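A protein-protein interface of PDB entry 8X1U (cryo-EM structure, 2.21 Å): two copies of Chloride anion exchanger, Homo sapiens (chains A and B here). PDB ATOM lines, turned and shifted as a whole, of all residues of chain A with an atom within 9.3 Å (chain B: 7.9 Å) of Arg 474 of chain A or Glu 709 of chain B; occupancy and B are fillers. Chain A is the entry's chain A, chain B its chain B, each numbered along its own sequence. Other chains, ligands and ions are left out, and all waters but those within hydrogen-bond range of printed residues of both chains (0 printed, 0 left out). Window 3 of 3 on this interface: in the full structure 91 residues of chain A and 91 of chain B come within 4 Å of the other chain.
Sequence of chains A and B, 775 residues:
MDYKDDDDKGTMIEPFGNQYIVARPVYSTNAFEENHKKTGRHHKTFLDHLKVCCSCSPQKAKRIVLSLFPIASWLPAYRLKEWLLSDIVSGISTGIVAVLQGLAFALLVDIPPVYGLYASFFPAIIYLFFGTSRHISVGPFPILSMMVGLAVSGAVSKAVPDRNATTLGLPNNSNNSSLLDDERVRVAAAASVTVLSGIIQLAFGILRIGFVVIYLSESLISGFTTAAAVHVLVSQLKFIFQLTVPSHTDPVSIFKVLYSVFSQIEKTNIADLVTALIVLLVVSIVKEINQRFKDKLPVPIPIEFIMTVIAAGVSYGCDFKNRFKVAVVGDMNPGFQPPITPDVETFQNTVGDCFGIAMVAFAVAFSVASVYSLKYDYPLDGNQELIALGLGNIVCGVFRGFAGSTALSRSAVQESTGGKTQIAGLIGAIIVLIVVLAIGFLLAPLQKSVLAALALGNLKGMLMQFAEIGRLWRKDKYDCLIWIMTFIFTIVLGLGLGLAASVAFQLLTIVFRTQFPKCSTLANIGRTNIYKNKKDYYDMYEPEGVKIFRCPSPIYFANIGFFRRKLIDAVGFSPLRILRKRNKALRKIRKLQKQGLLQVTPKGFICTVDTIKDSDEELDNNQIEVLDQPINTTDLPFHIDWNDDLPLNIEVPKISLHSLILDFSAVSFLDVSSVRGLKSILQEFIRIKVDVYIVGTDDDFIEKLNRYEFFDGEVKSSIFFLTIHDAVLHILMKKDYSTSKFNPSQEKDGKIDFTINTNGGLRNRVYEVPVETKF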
ATOM      1  N   ALA A 467       2.234   3.623   6.690  1.00  0.00           N
ATOM      2  CA  ALA A 467       3.094   4.128   7.748  1.00  0.00           C
ATOM      3  C   ALA A 467       2.330   4.468   9.016  1.00  0.00           C
ATOM      4  O   ALA A 467       2.957   4.652  10.062  1.00  0.00           O
ATOM      5  CB  ALA A 467       3.851   5.361   7.261  1.00  0.00           C
ATOM      6  N   GLU A 468       1.002   4.556   8.949  1.00  0.00           N
ATOM      7  CA  GLU A 468       0.217   4.894  10.128  1.00  0.00           C
ATOM      8  C   GLU A 468       0.150   3.750  11.125  1.00  0.00           C
ATOM      9  O   GLU A 468      -0.203   3.980  12.284  1.00  0.00           O
ATOM     10  CB  GLU A 468      -1.192   5.313   9.719  1.00  0.00           C
ATOM     11  CG  GLU A 468      -1.354   6.809   9.552  1.00  0.00           C
ATOM     12  CD  GLU A 468      -1.890   7.480  10.802  1.00  0.00           C
ATOM     13  OE1 GLU A 468      -3.009   7.134  11.230  1.00  0.00           O
ATOM     14  OE2 GLU A 468      -1.194   8.355  11.358  1.00  0.00           O
ATOM     15  N   ILE A 469       0.505   2.534  10.713  1.00  0.00           N
ATOM     16  CA  ILE A 469       0.480   1.397  11.630  1.00  0.00           C
ATOM     17  C   ILE A 469       1.426   1.633  12.802  1.00  0.00           C
ATOM     18  O   ILE A 469       1.023   1.565  13.966  1.00  0.00           O
ATOM     19  CB  ILE A 469       0.822   0.097  10.884  1.00  0.00           C
ATOM     20  CG1 ILE A 469      -0.156  -0.131   9.737  1.00  0.00           C
ATOM     21  CG2 ILE A 469       0.797  -1.079  11.835  1.00  0.00           C
ATOM     22  CD1 ILE A 469       0.164  -1.345   8.916  1.00  0.00           C
ATOM     23  N   GLY A 470       2.699   1.860  12.508  1.00  0.00           N
ATOM     24  CA  GLY A 470       3.679   2.035  13.560  1.00  0.00           C
ATOM     25  C   GLY A 470       3.429   3.250  14.411  1.00  0.00           C
ATOM     26  O   GLY A 470       3.662   3.230  15.619  1.00  0.00           O
ATOM     27  N   ARG A 471       2.954   4.315  13.790  1.00  0.00           N
ATOM     28  CA  ARG A 471       2.658   5.527  14.526  1.00  0.00           C
ATOM     29  C   ARG A 471       1.573   5.293  15.572  1.00  0.00           C
ATOM     30  O   ARG A 471       1.729   5.682  16.724  1.00  0.00           O
ATOM     31  CB  ARG A 471       2.250   6.632  13.556  1.00  0.00           C
ATOM     32  CG  ARG A 471       3.378   7.115  12.666  1.00  0.00           C
ATOM     33  CD  ARG A 471       2.996   8.393  11.940  1.00  0.00           C
ATOM     34  NE  ARG A 471       2.080   8.152  10.832  1.00  0.00           N
ATOM     35  CZ  ARG A 471       2.466   8.003   9.571  1.00  0.00           C
ATOM     36  NH1 ARG A 471       1.568   7.789   8.620  1.00  0.00           N
ATOM     37  NH2 ARG A 471       3.752   8.073   9.259  1.00  0.00           N
ATOM     38  N   LEU A 472       0.485   4.645  15.179  1.00  0.00           N
ATOM     39  CA  LEU A 472      -0.613   4.391  16.104  1.00  0.00           C
ATOM     40  C   LEU A 472      -0.203   3.402  17.175  1.00  0.00           C
ATOM     41  O   LEU A 472      -0.685   3.471  18.300  1.00  0.00           O
ATOM     42  CB  LEU A 472      -1.844   3.888  15.351  1.00  0.00           C
ATOM     43  CG  LEU A 472      -2.454   4.849  14.329  1.00  0.00           C
ATOM     44  CD1 LEU A 472      -3.585   4.185  13.560  1.00  0.00           C
ATOM     45  CD2 LEU A 472      -2.933   6.120  15.010  1.00  0.00           C
ATOM     46  N   TRP A 473       0.685   2.479  16.833  1.00  0.00           N
ATOM     47  CA  TRP A 473       1.163   1.517  17.807  1.00  0.00           C
ATOM     48  C   TRP A 473       1.820   2.228  18.974  1.00  0.00           C
ATOM     49  O   TRP A 473       1.647   1.838  20.121  1.00  0.00           O
ATOM     50  CB  TRP A 473       2.161   0.573  17.159  1.00  0.00           C
ATOM     51  CG  TRP A 473       2.795  -0.364  18.115  1.00  0.00           C
ATOM     52  CD1 TRP A 473       4.016  -0.235  18.702  1.00  0.00           C
ATOM     53  CD2 TRP A 473       2.239  -1.584  18.609  1.00  0.00           C
ATOM     54  NE1 TRP A 473       4.259  -1.300  19.529  1.00  0.00           N
ATOM     55  CE2 TRP A 473       3.181  -2.145  19.489  1.00  0.00           C
ATOM     56  CE3 TRP A 473       1.034  -2.258  18.390  1.00  0.00           C
ATOM     57  CZ2 TRP A 473       2.958  -3.347  20.151  1.00  0.00           C
ATOM     58  CZ3 TRP A 473       0.817  -3.449  19.046  1.00  0.00           C
ATOM     59  CH2 TRP A 473       1.772  -3.983  19.917  1.00  0.00           C
ATOM     60  N   ARG A 474       2.574   3.276  18.681  1.00  0.00           N
ATOM     61  CA  ARG A 474       3.228   4.037  19.735  1.00  0.00           C
ATOM     62  C   ARG A 474       2.291   4.976  20.489  1.00  0.00           C
ATOM     63  O   ARG A 474       2.484   5.204  21.677  1.00  0.00           O
ATOM     64  CB  ARG A 474       4.388   4.837  19.148  1.00  0.00           C
ATOM     65  CG  ARG A 474       5.396   4.003  18.382  1.00  0.00           C
ATOM     66  CD  ARG A 474       6.593   4.850  17.988  1.00  0.00           C
ATOM     67  NE  ARG A 474       6.187   6.066  17.292  1.00  0.00           N
ATOM     68  CZ  ARG A 474       6.079   6.170  15.972  1.00  0.00           C
ATOM     69  NH1 ARG A 474       5.702   7.317  15.426  1.00  0.00           N
ATOM     70  NH2 ARG A 474       6.352   5.130  15.198  1.00  0.00           N
ATOM     71  N   LYS A 475       1.276   5.512  19.826  1.00  0.00           N
ATOM     72  CA  LYS A 475       0.402   6.501  20.466  1.00  0.00           C
ATOM     73  C   LYS A 475      -0.848   5.939  21.141  1.00  0.00           C
ATOM     74  O   LYS A 475      -1.125   6.272  22.285  1.00  0.00           O
ATOM     75  CB  LYS A 475      -0.010   7.548  19.429  1.00  0.00           C
ATOM     76  CG  LYS A 475       1.160   8.295  18.821  1.00  0.00           C
ATOM     77  CD  LYS A 475       0.707   9.191  17.685  1.00  0.00           C
ATOM     78  CE  LYS A 475       1.895   9.860  17.016  1.00  0.00           C
ATOM     79  NZ  LYS A 475       1.482  10.690  15.852  1.00  0.00           N
ATOM     80  N   ASP A 476      -1.606   5.108  20.437  1.00  0.00           N
ATOM     81  CA  ASP A 476      -2.841   4.560  20.977  1.00  0.00           C
ATOM     82  C   ASP A 476      -3.084   3.218  20.343  1.00  0.00           C
ATOM     83  O   ASP A 476      -3.426   3.135  19.169  1.00  0.00           O
ATOM     84  CB  ASP A 476      -4.014   5.503  20.707  1.00  0.00           C
ATOM     85  CG  ASP A 476      -5.295   5.066  21.389  1.00  0.00           C
ATOM     86  OD1 ASP A 476      -5.462   3.862  21.663  1.00  0.00           O
ATOM     87  OD2 ASP A 476      -6.146   5.939  21.645  1.00  0.00           O
ATOM     88  N   LYS A 477      -2.939   2.160  21.118  1.00  0.00           N
ATOM     89  CA  LYS A 477      -3.084   0.822  20.571  1.00  0.00           C
ATOM     90  C   LYS A 477      -4.528   0.481  20.244  1.00  0.00           C
ATOM     91  O   LYS A 477      -4.773  -0.457  19.502  1.00  0.00           O
ATOM     92  CB  LYS A 477      -2.469  -0.206  21.520  1.00  0.00           C
ATOM     93  CG  LYS A 477      -0.985   0.015  21.753  1.00  0.00           C
ATOM     94  CD  LYS A 477      -0.334  -1.182  22.419  1.00  0.00           C
ATOM     95  CE  LYS A 477       1.105  -0.878  22.793  1.00  0.00           C
ATOM     96  NZ  LYS A 477       1.882  -0.371  21.633  1.00  0.00           N
ATOM     97  N   TYR A 478      -5.485   1.235  20.773  1.00  0.00           N
ATOM     98  CA  TYR A 478      -6.867   0.991  20.374  1.00  0.00           C
ATOM     99  C   TYR A 478      -7.121   1.508  18.967  1.00  0.00           C
ATOM    100  O   TYR A 478      -7.830   0.871  18.183  1.00  0.00           O
ATOM    101  CB  TYR A 478      -7.830   1.640  21.364  1.00  0.00           C
ATOM    102  CG  TYR A 478      -7.717   1.114  22.773  1.00  0.00           C
ATOM    103  CD1 TYR A 478      -8.344  -0.058  23.148  1.00  0.00           C
ATOM    104  CD2 TYR A 478      -6.984   1.799  23.728  1.00  0.00           C
ATOM    105  CE1 TYR A 478      -8.241  -0.539  24.432  1.00  0.00           C
ATOM    106  CE2 TYR A 478      -6.877   1.328  25.013  1.00  0.00           C
ATOM    107  CZ  TYR A 478      -7.508   0.159  25.361  1.00  0.00           C
ATOM    108  OH  TYR A 478      -7.404  -0.312  26.648  1.00  0.00           O
ATOM    109  N   ASP A 479      -6.518   2.640  18.614  1.00  0.00           N
ATOM    110  CA  ASP A 479      -6.656   3.147  17.255  1.00  0.00           C
ATOM    111  C   ASP A 479      -5.797   2.357  16.278  1.00  0.00           C
ATOM    112  O   ASP A 479      -6.164   2.202  15.110  1.00  0.00           O
ATOM    113  CB  ASP A 479      -6.310   4.631  17.221  1.00  0.00           C
ATOM    114  CG  ASP A 479      -7.364   5.485  17.899  1.00  0.00           C
ATOM    115  OD1 ASP A 479      -8.494   5.575  17.380  1.00  0.00           O
ATOM    116  OD2 ASP A 479      -7.061   6.070  18.953  1.00  0.00           O
ATOM    117  N   CYS A 480      -4.655   1.838  16.733  1.00  0.00           N
ATOM    118  CA  CYS A 480      -3.910   0.877  15.924  1.00  0.00           C
ATOM    119  C   CYS A 480      -4.739  -0.372  15.662  1.00  0.00           C
ATOM    120  O   CYS A 480      -4.708  -0.932  14.560  1.00  0.00           O
ATOM    121  CB  CYS A 480      -2.602   0.504  16.614  1.00  0.00           C
ATOM    122  SG  CYS A 480      -1.300  -0.033  15.498  1.00  0.00           S
ATOM    123  N   LEU A 481      -5.482  -0.826  16.669  1.00  0.00           N
ATOM    124  CA  LEU A 481      -6.367  -1.966  16.482  1.00  0.00           C
ATOM    125  C   LEU A 481      -7.473  -1.641  15.490  1.00  0.00           C
ATOM    126  O   LEU A 481      -7.818  -2.471  14.646  1.00  0.00           O
ATOM    127  CB  LEU A 481      -6.944  -2.387  17.833  1.00  0.00           C
ATOM    128  CG  LEU A 481      -7.697  -3.707  17.951  1.00  0.00           C
ATOM    129  CD1 LEU A 481      -6.759  -4.887  17.801  1.00  0.00           C
ATOM    130  CD2 LEU A 481      -8.403  -3.749  19.283  1.00  0.00           C
ATOM    131  N   VAL B 672      -6.841   9.121  19.193  1.00  0.00           N
ATOM    132  CA  VAL B 672      -5.961   9.806  18.256  1.00  0.00           C
ATOM    133  C   VAL B 672      -6.672  10.976  17.583  1.00  0.00           C
ATOM    134  O   VAL B 672      -6.109  12.055  17.456  1.00  0.00           O
ATOM    135  CB  VAL B 672      -5.384   8.837  17.201  1.00  0.00           C
ATOM    136  CG1 VAL B 672      -4.613   7.721  17.878  1.00  0.00           C
ATOM    137  CG2 VAL B 672      -6.508   8.259  16.361  1.00  0.00           C
ATOM    138  N   VAL B 675      -7.014  13.907  20.159  1.00  0.00           N
ATOM    139  CA  VAL B 675      -5.768  14.544  20.530  1.00  0.00           C
ATOM    140  C   VAL B 675      -5.346  15.465  19.400  1.00  0.00           C
ATOM    141  O   VAL B 675      -4.860  16.561  19.645  1.00  0.00           O
ATOM    142  CB  VAL B 675      -4.651  13.531  20.888  1.00  0.00           C
ATOM    143  CG1 VAL B 675      -3.338  14.248  21.149  1.00  0.00           C
ATOM    144  CG2 VAL B 675      -5.047  12.671  22.076  1.00  0.00           C
ATOM    145  N   LYS B 679      -4.999  19.475  19.798  1.00  0.00           N
ATOM    146  CA  LYS B 679      -3.739  20.155  19.563  1.00  0.00           C
ATOM    147  C   LYS B 679      -3.935  21.313  18.605  1.00  0.00           C
ATOM    148  O   LYS B 679      -3.420  22.401  18.834  1.00  0.00           O
ATOM    149  CB  LYS B 679      -2.686  19.190  19.025  1.00  0.00           C
ATOM    150  CG  LYS B 679      -1.297  19.800  18.993  1.00  0.00           C
ATOM    151  CD  LYS B 679      -0.221  18.761  18.752  1.00  0.00           C
ATOM    152  CE  LYS B 679       1.156  19.398  18.796  1.00  0.00           C
ATOM    153  NZ  LYS B 679       2.234  18.395  18.589  1.00  0.00           N
ATOM    154  N   GLU B 703       0.116  11.357  31.466  1.00  0.00           N
ATOM    155  CA  GLU B 703       1.019  10.288  31.086  1.00  0.00           C
ATOM    156  C   GLU B 703       0.685   9.772  29.677  1.00  0.00           C
ATOM    157  O   GLU B 703       1.571   9.619  28.853  1.00  0.00           O
ATOM    158  CB  GLU B 703       0.953   9.163  32.111  1.00  0.00           C
ATOM    159  CG  GLU B 703       2.209   8.324  32.186  1.00  0.00           C
ATOM    160  CD  GLU B 703       2.424   7.496  30.940  1.00  0.00           C
ATOM    161  OE1 GLU B 703       3.439   7.716  30.241  1.00  0.00           O
ATOM    162  OE2 GLU B 703       1.568   6.632  30.652  1.00  0.00           O
ATOM    163  N   LYS B 704      -0.590   9.504  29.416  1.00  0.00           N
ATOM    164  CA  LYS B 704      -1.062   9.031  28.119  1.00  0.00           C
ATOM    165  C   LYS B 704      -0.903  10.087  27.033  1.00  0.00           C
ATOM    166  O   LYS B 704      -0.562   9.760  25.904  1.00  0.00           O
ATOM    167  CB  LYS B 704      -2.519   8.581  28.208  1.00  0.00           C
ATOM    168  CG  LYS B 704      -2.765   7.431  29.165  1.00  0.00           C
ATOM    169  CD  LYS B 704      -4.204   6.956  29.076  1.00  0.00           C
ATOM    170  CE  LYS B 704      -4.515   5.932  30.154  1.00  0.00           C
ATOM    171  NZ  LYS B 704      -4.352   6.511  31.516  1.00  0.00           N
ATOM    172  N   LEU B 705      -1.129  11.347  27.370  1.00  0.00           N
ATOM    173  CA  LEU B 705      -0.982  12.430  26.403  1.00  0.00           C
ATOM    174  C   LEU B 705       0.457  12.545  25.921  1.00  0.00           C
ATOM    175  O   LEU B 705       0.699  12.945  24.789  1.00  0.00           O
ATOM    176  CB  LEU B 705      -1.459  13.745  27.010  1.00  0.00           C
ATOM    177  CG  LEU B 705      -1.901  14.856  26.064  1.00  0.00           C
ATOM    178  CD1 LEU B 705      -2.892  14.326  25.040  1.00  0.00           C
ATOM    179  CD2 LEU B 705      -2.513  15.991  26.869  1.00  0.00           C
ATOM    180  N   ASN B 706       1.415  12.210  26.775  1.00  0.00           N
ATOM    181  CA  ASN B 706       2.819  12.218  26.369  1.00  0.00           C
ATOM    182  C   ASN B 706       3.095  11.184  25.282  1.00  0.00           C
ATOM    183  O   ASN B 706       3.942  11.399  24.423  1.00  0.00           O
ATOM    184  CB  ASN B 706       3.727  11.952  27.568  1.00  0.00           C
ATOM    185  CG  ASN B 706       3.580  12.991  28.655  1.00  0.00           C
ATOM    186  OD1 ASN B 706       3.404  14.174  28.379  1.00  0.00           O
ATOM    187  ND2 ASN B 706       3.662  12.553  29.904  1.00  0.00           N
ATOM    188  N   ARG B 707       2.372  10.075  25.301  1.00  0.00           N
ATOM    189  CA  ARG B 707       2.552   9.049  24.293  1.00  0.00           C
ATOM    190  C   ARG B 707       1.999   9.452  22.937  1.00  0.00           C
ATOM    191  O   ARG B 707       2.358   8.866  21.933  1.00  0.00           O
ATOM    192  CB  ARG B 707       1.920   7.741  24.738  1.00  0.00           C
ATOM    193  CG  ARG B 707       2.649   7.103  25.894  1.00  0.00           C
ATOM    194  CD  ARG B 707       2.488   5.604  25.848  1.00  0.00           C
ATOM    195  NE  ARG B 707       1.084   5.230  25.831  1.00  0.00           N
ATOM    196  CZ  ARG B 707       0.354   5.044  26.921  1.00  0.00           C
ATOM    197  NH1 ARG B 707       0.905   5.205  28.114  1.00  0.00           N
ATOM    198  NH2 ARG B 707      -0.922   4.704  26.816  1.00  0.00           N
ATOM    199  N   TYR B 708       1.111  10.436  22.917  1.00  0.00           N
ATOM    200  CA  TYR B 708       0.531  10.915  21.668  1.00  0.00           C
ATOM    201  C   TYR B 708       1.384  11.972  21.014  1.00  0.00           C
ATOM    202  O   TYR B 708       1.016  12.495  19.971  1.00  0.00           O
ATOM    203  CB  TYR B 708      -0.850  11.514  21.904  1.00  0.00           C
ATOM    204  CG  TYR B 708      -1.953  10.526  22.177  1.00  0.00           C
ATOM    205  CD1 TYR B 708      -2.330  10.222  23.474  1.00  0.00           C
ATOM    206  CD2 TYR B 708      -2.642   9.921  21.134  1.00  0.00           C
ATOM    207  CE1 TYR B 708      -3.351   9.330  23.728  1.00  0.00           C
ATOM    208  CE2 TYR B 708      -3.665   9.027  21.380  1.00  0.00           C
ATOM    209  CZ  TYR B 708      -4.014   8.735  22.678  1.00  0.00           C
ATOM    210  OH  TYR B 708      -5.030   7.849  22.937  1.00  0.00           O
ATOM    211  N   GLU B 709       2.514  12.307  21.621  1.00  0.00           N
ATOM    212  CA  GLU B 709       3.365  13.368  21.093  1.00  0.00           C
ATOM    213  C   GLU B 709       2.583  14.666  21.030  1.00  0.00           C
ATOM    214  O   GLU B 709       2.692  15.416  20.063  1.00  0.00           O
ATOM    215  CB  GLU B 709       3.912  12.987  19.720  1.00  0.00           C
ATOM    216  CG  GLU B 709       4.576  11.620  19.690  1.00  0.00           C
ATOM    217  CD  GLU B 709       5.023  11.214  18.300  1.00  0.00           C
ATOM    218  OE1 GLU B 709       5.514  10.076  18.143  1.00  0.00           O
ATOM    219  OE2 GLU B 709       4.882  12.030  17.364  1.00  0.00           O
ATOM    220  N   PHE B 710       1.801  14.938  22.063  1.00  0.00           N
ATOM    221  CA  PHE B 710       0.980  16.138  22.096  1.00  0.00           C
ATOM    222  C   PHE B 710       1.799  17.369  22.409  1.00  0.00           C
ATOM    223  O   PHE B 710       1.549  18.436  21.865  1.00  0.00           O
ATOM    224  CB  PHE B 710      -0.106  15.951  23.155  1.00  0.00           C
ATOM    225  CG  PHE B 710      -1.076  17.086  23.256  1.00  0.00           C
ATOM    226  CD1 PHE B 710      -0.999  17.984  24.304  1.00  0.00           C
ATOM    227  CD2 PHE B 710      -2.081  17.238  22.319  1.00  0.00           C
ATOM    228  CE1 PHE B 710      -1.899  19.023  24.409  1.00  0.00           C
ATOM    229  CE2 PHE B 710      -2.984  18.275  22.417  1.00  0.00           C
ATOM    230  CZ  PHE B 710      -2.893  19.169  23.462  1.00  0.00           C
ATOM    231  N   PHE B 711       2.783  17.228  23.284  1.00  0.00           N
ATOM    232  CA  PHE B 711       3.564  18.384  23.705  1.00  0.00           C
ATOM    233  C   PHE B 711       4.730  18.695  22.791  1.00  0.00           C
ATOM    234  O   PHE B 711       5.346  17.795  22.235  1.00  0.00           O
ATOM    235  CB  PHE B 711       4.043  18.195  25.145  1.00  0.00           C
ATOM    236  CG  PHE B 711       2.923  18.013  26.125  1.00  0.00           C
ATOM    237  CD1 PHE B 711       2.110  19.079  26.467  1.00  0.00           C
ATOM    238  CD2 PHE B 711       2.671  16.776  26.688  1.00  0.00           C
ATOM    239  CE1 PHE B 711       1.073  18.916  27.362  1.00  0.00           C
ATOM    240  CE2 PHE B 711       1.635  16.605  27.584  1.00  0.00           C
ATOM    241  CZ  PHE B 711       0.835  17.678  27.922  1.00  0.00           C
ATOM    242  N   ASP B 712       5.031  19.976  22.638  1.00  0.00           N
ATOM    243  CA  ASP B 712       6.110  20.399  21.759  1.00  0.00           C
ATOM    244  C   ASP B 712       6.498  21.807  22.160  1.00  0.00           C
ATOM    245  O   ASP B 712       6.213  22.235  23.273  1.00  0.00           O
ATOM    246  CB  ASP B 712       5.636  20.440  20.307  1.00  0.00           C
ATOM    247  CG  ASP B 712       4.434  21.343  20.107  1.00  0.00           C
ATOM    248  OD1 ASP B 712       3.833  21.778  21.108  1.00  0.00           O
ATOM    249  OD2 ASP B 712       4.083  21.613  18.941  1.00  0.00           O
ATOM    250  N   VAL B 715       2.937  23.981  22.437  1.00  0.00           N
ATOM    251  CA  VAL B 715       2.075  23.424  23.468  1.00  0.00           C
ATOM    252  C   VAL B 715       2.955  22.711  24.462  1.00  0.00           C
ATOM    253  O   VAL B 715       3.620  21.747  24.114  1.00  0.00           O
ATOM    254  CB  VAL B 715       1.033  22.462  22.881  1.00  0.00           C
ATOM    255  CG1 VAL B 715       0.120  21.935  23.977  1.00  0.00           C
ATOM    256  CG2 VAL B 715       0.227  23.152  21.795  1.00  0.00           C
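The guanidinium group of Arg 474 of chain A lies within salt-bridge range of the side-chain carboxylate of Glu 709 of chain B (3.9 Å). The side-chain amino group of Lys 475 of chain A lies within salt-bridge range of the side-chain carboxylate of Glu 709 of chain B. OD2 of Asp 476 of chain A lies within hydrogen-bond range of OH of Tyr 708 of chain B (2.6 Å). The side-chain carboxylate (OD2) of Asp 479 of chain A is in hydrogen-bond range of the backbone NH (N) of Val 672 of chain B (3.1 Å).
O of Gly 470 of chain A lies within hydrogen-bond range of NH2 of Arg 474 of chain A (3.3 Å). The side-chain carboxylate of Asp 476 of chain A sits at hydrogen-bond distance from the backbone NH of Tyr 478 of chain A, 2.8 Å away. OD1 of Asp 476 of chain A sits at hydrogen-bond distance from N of Asp 479 of chain A (3.5 Å). The side-chain amino group (NZ) of Lys 679 of chain B lies within hydrogen-bond range of the backbone carbonyl oxygen (O) of Glu 709 of chain B, 3.4 Å away. The guanidinium group of Arg 707 of chain B lies within salt-bridge range of the side-chain carboxylate of Glu 703 of chain B, at 3.0 Å.
Among the printed residues, merely in contact across the chains: Leu 472 of chain A with Val 672 of chain B, Arg 474 of chain A with Arg 707 of chain B, Lys 475 of chain A with Arg 707 of chain B, Lys 475 of chain A with Tyr 708 of chain B and Asp 476 of chain A with Val 672 of chain B.
Arg 474 of chain A touches just these residues of chain B: Arg 707 (3.7 Å) and Glu 709 (3.9 Å). Of chain A, only Arg 474 (3.9 Å) and Lys 475 (3.6 Å) come within 4 Å of Glu 709 of chain B. Printed residues of chain B within 4 Å of Asp 476 of chain A: Val 672 and Tyr 708. Of the printed residues of chain B, Asp 479 of chain A touches Val 672 (3.1 Å). Of the printed residues of chain B, Leu 472 of chain A touches Val 672 (3.7 Å). The nearest residue of chain A that does not touch Glu 709 of chain B is Arg 471 of chain A (6.0 Å). The nearest printed residue of chain B that does not touch Asp 479 of chain A is Tyr 708 of chain B (4.8 Å).
No position is printed for both chains.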
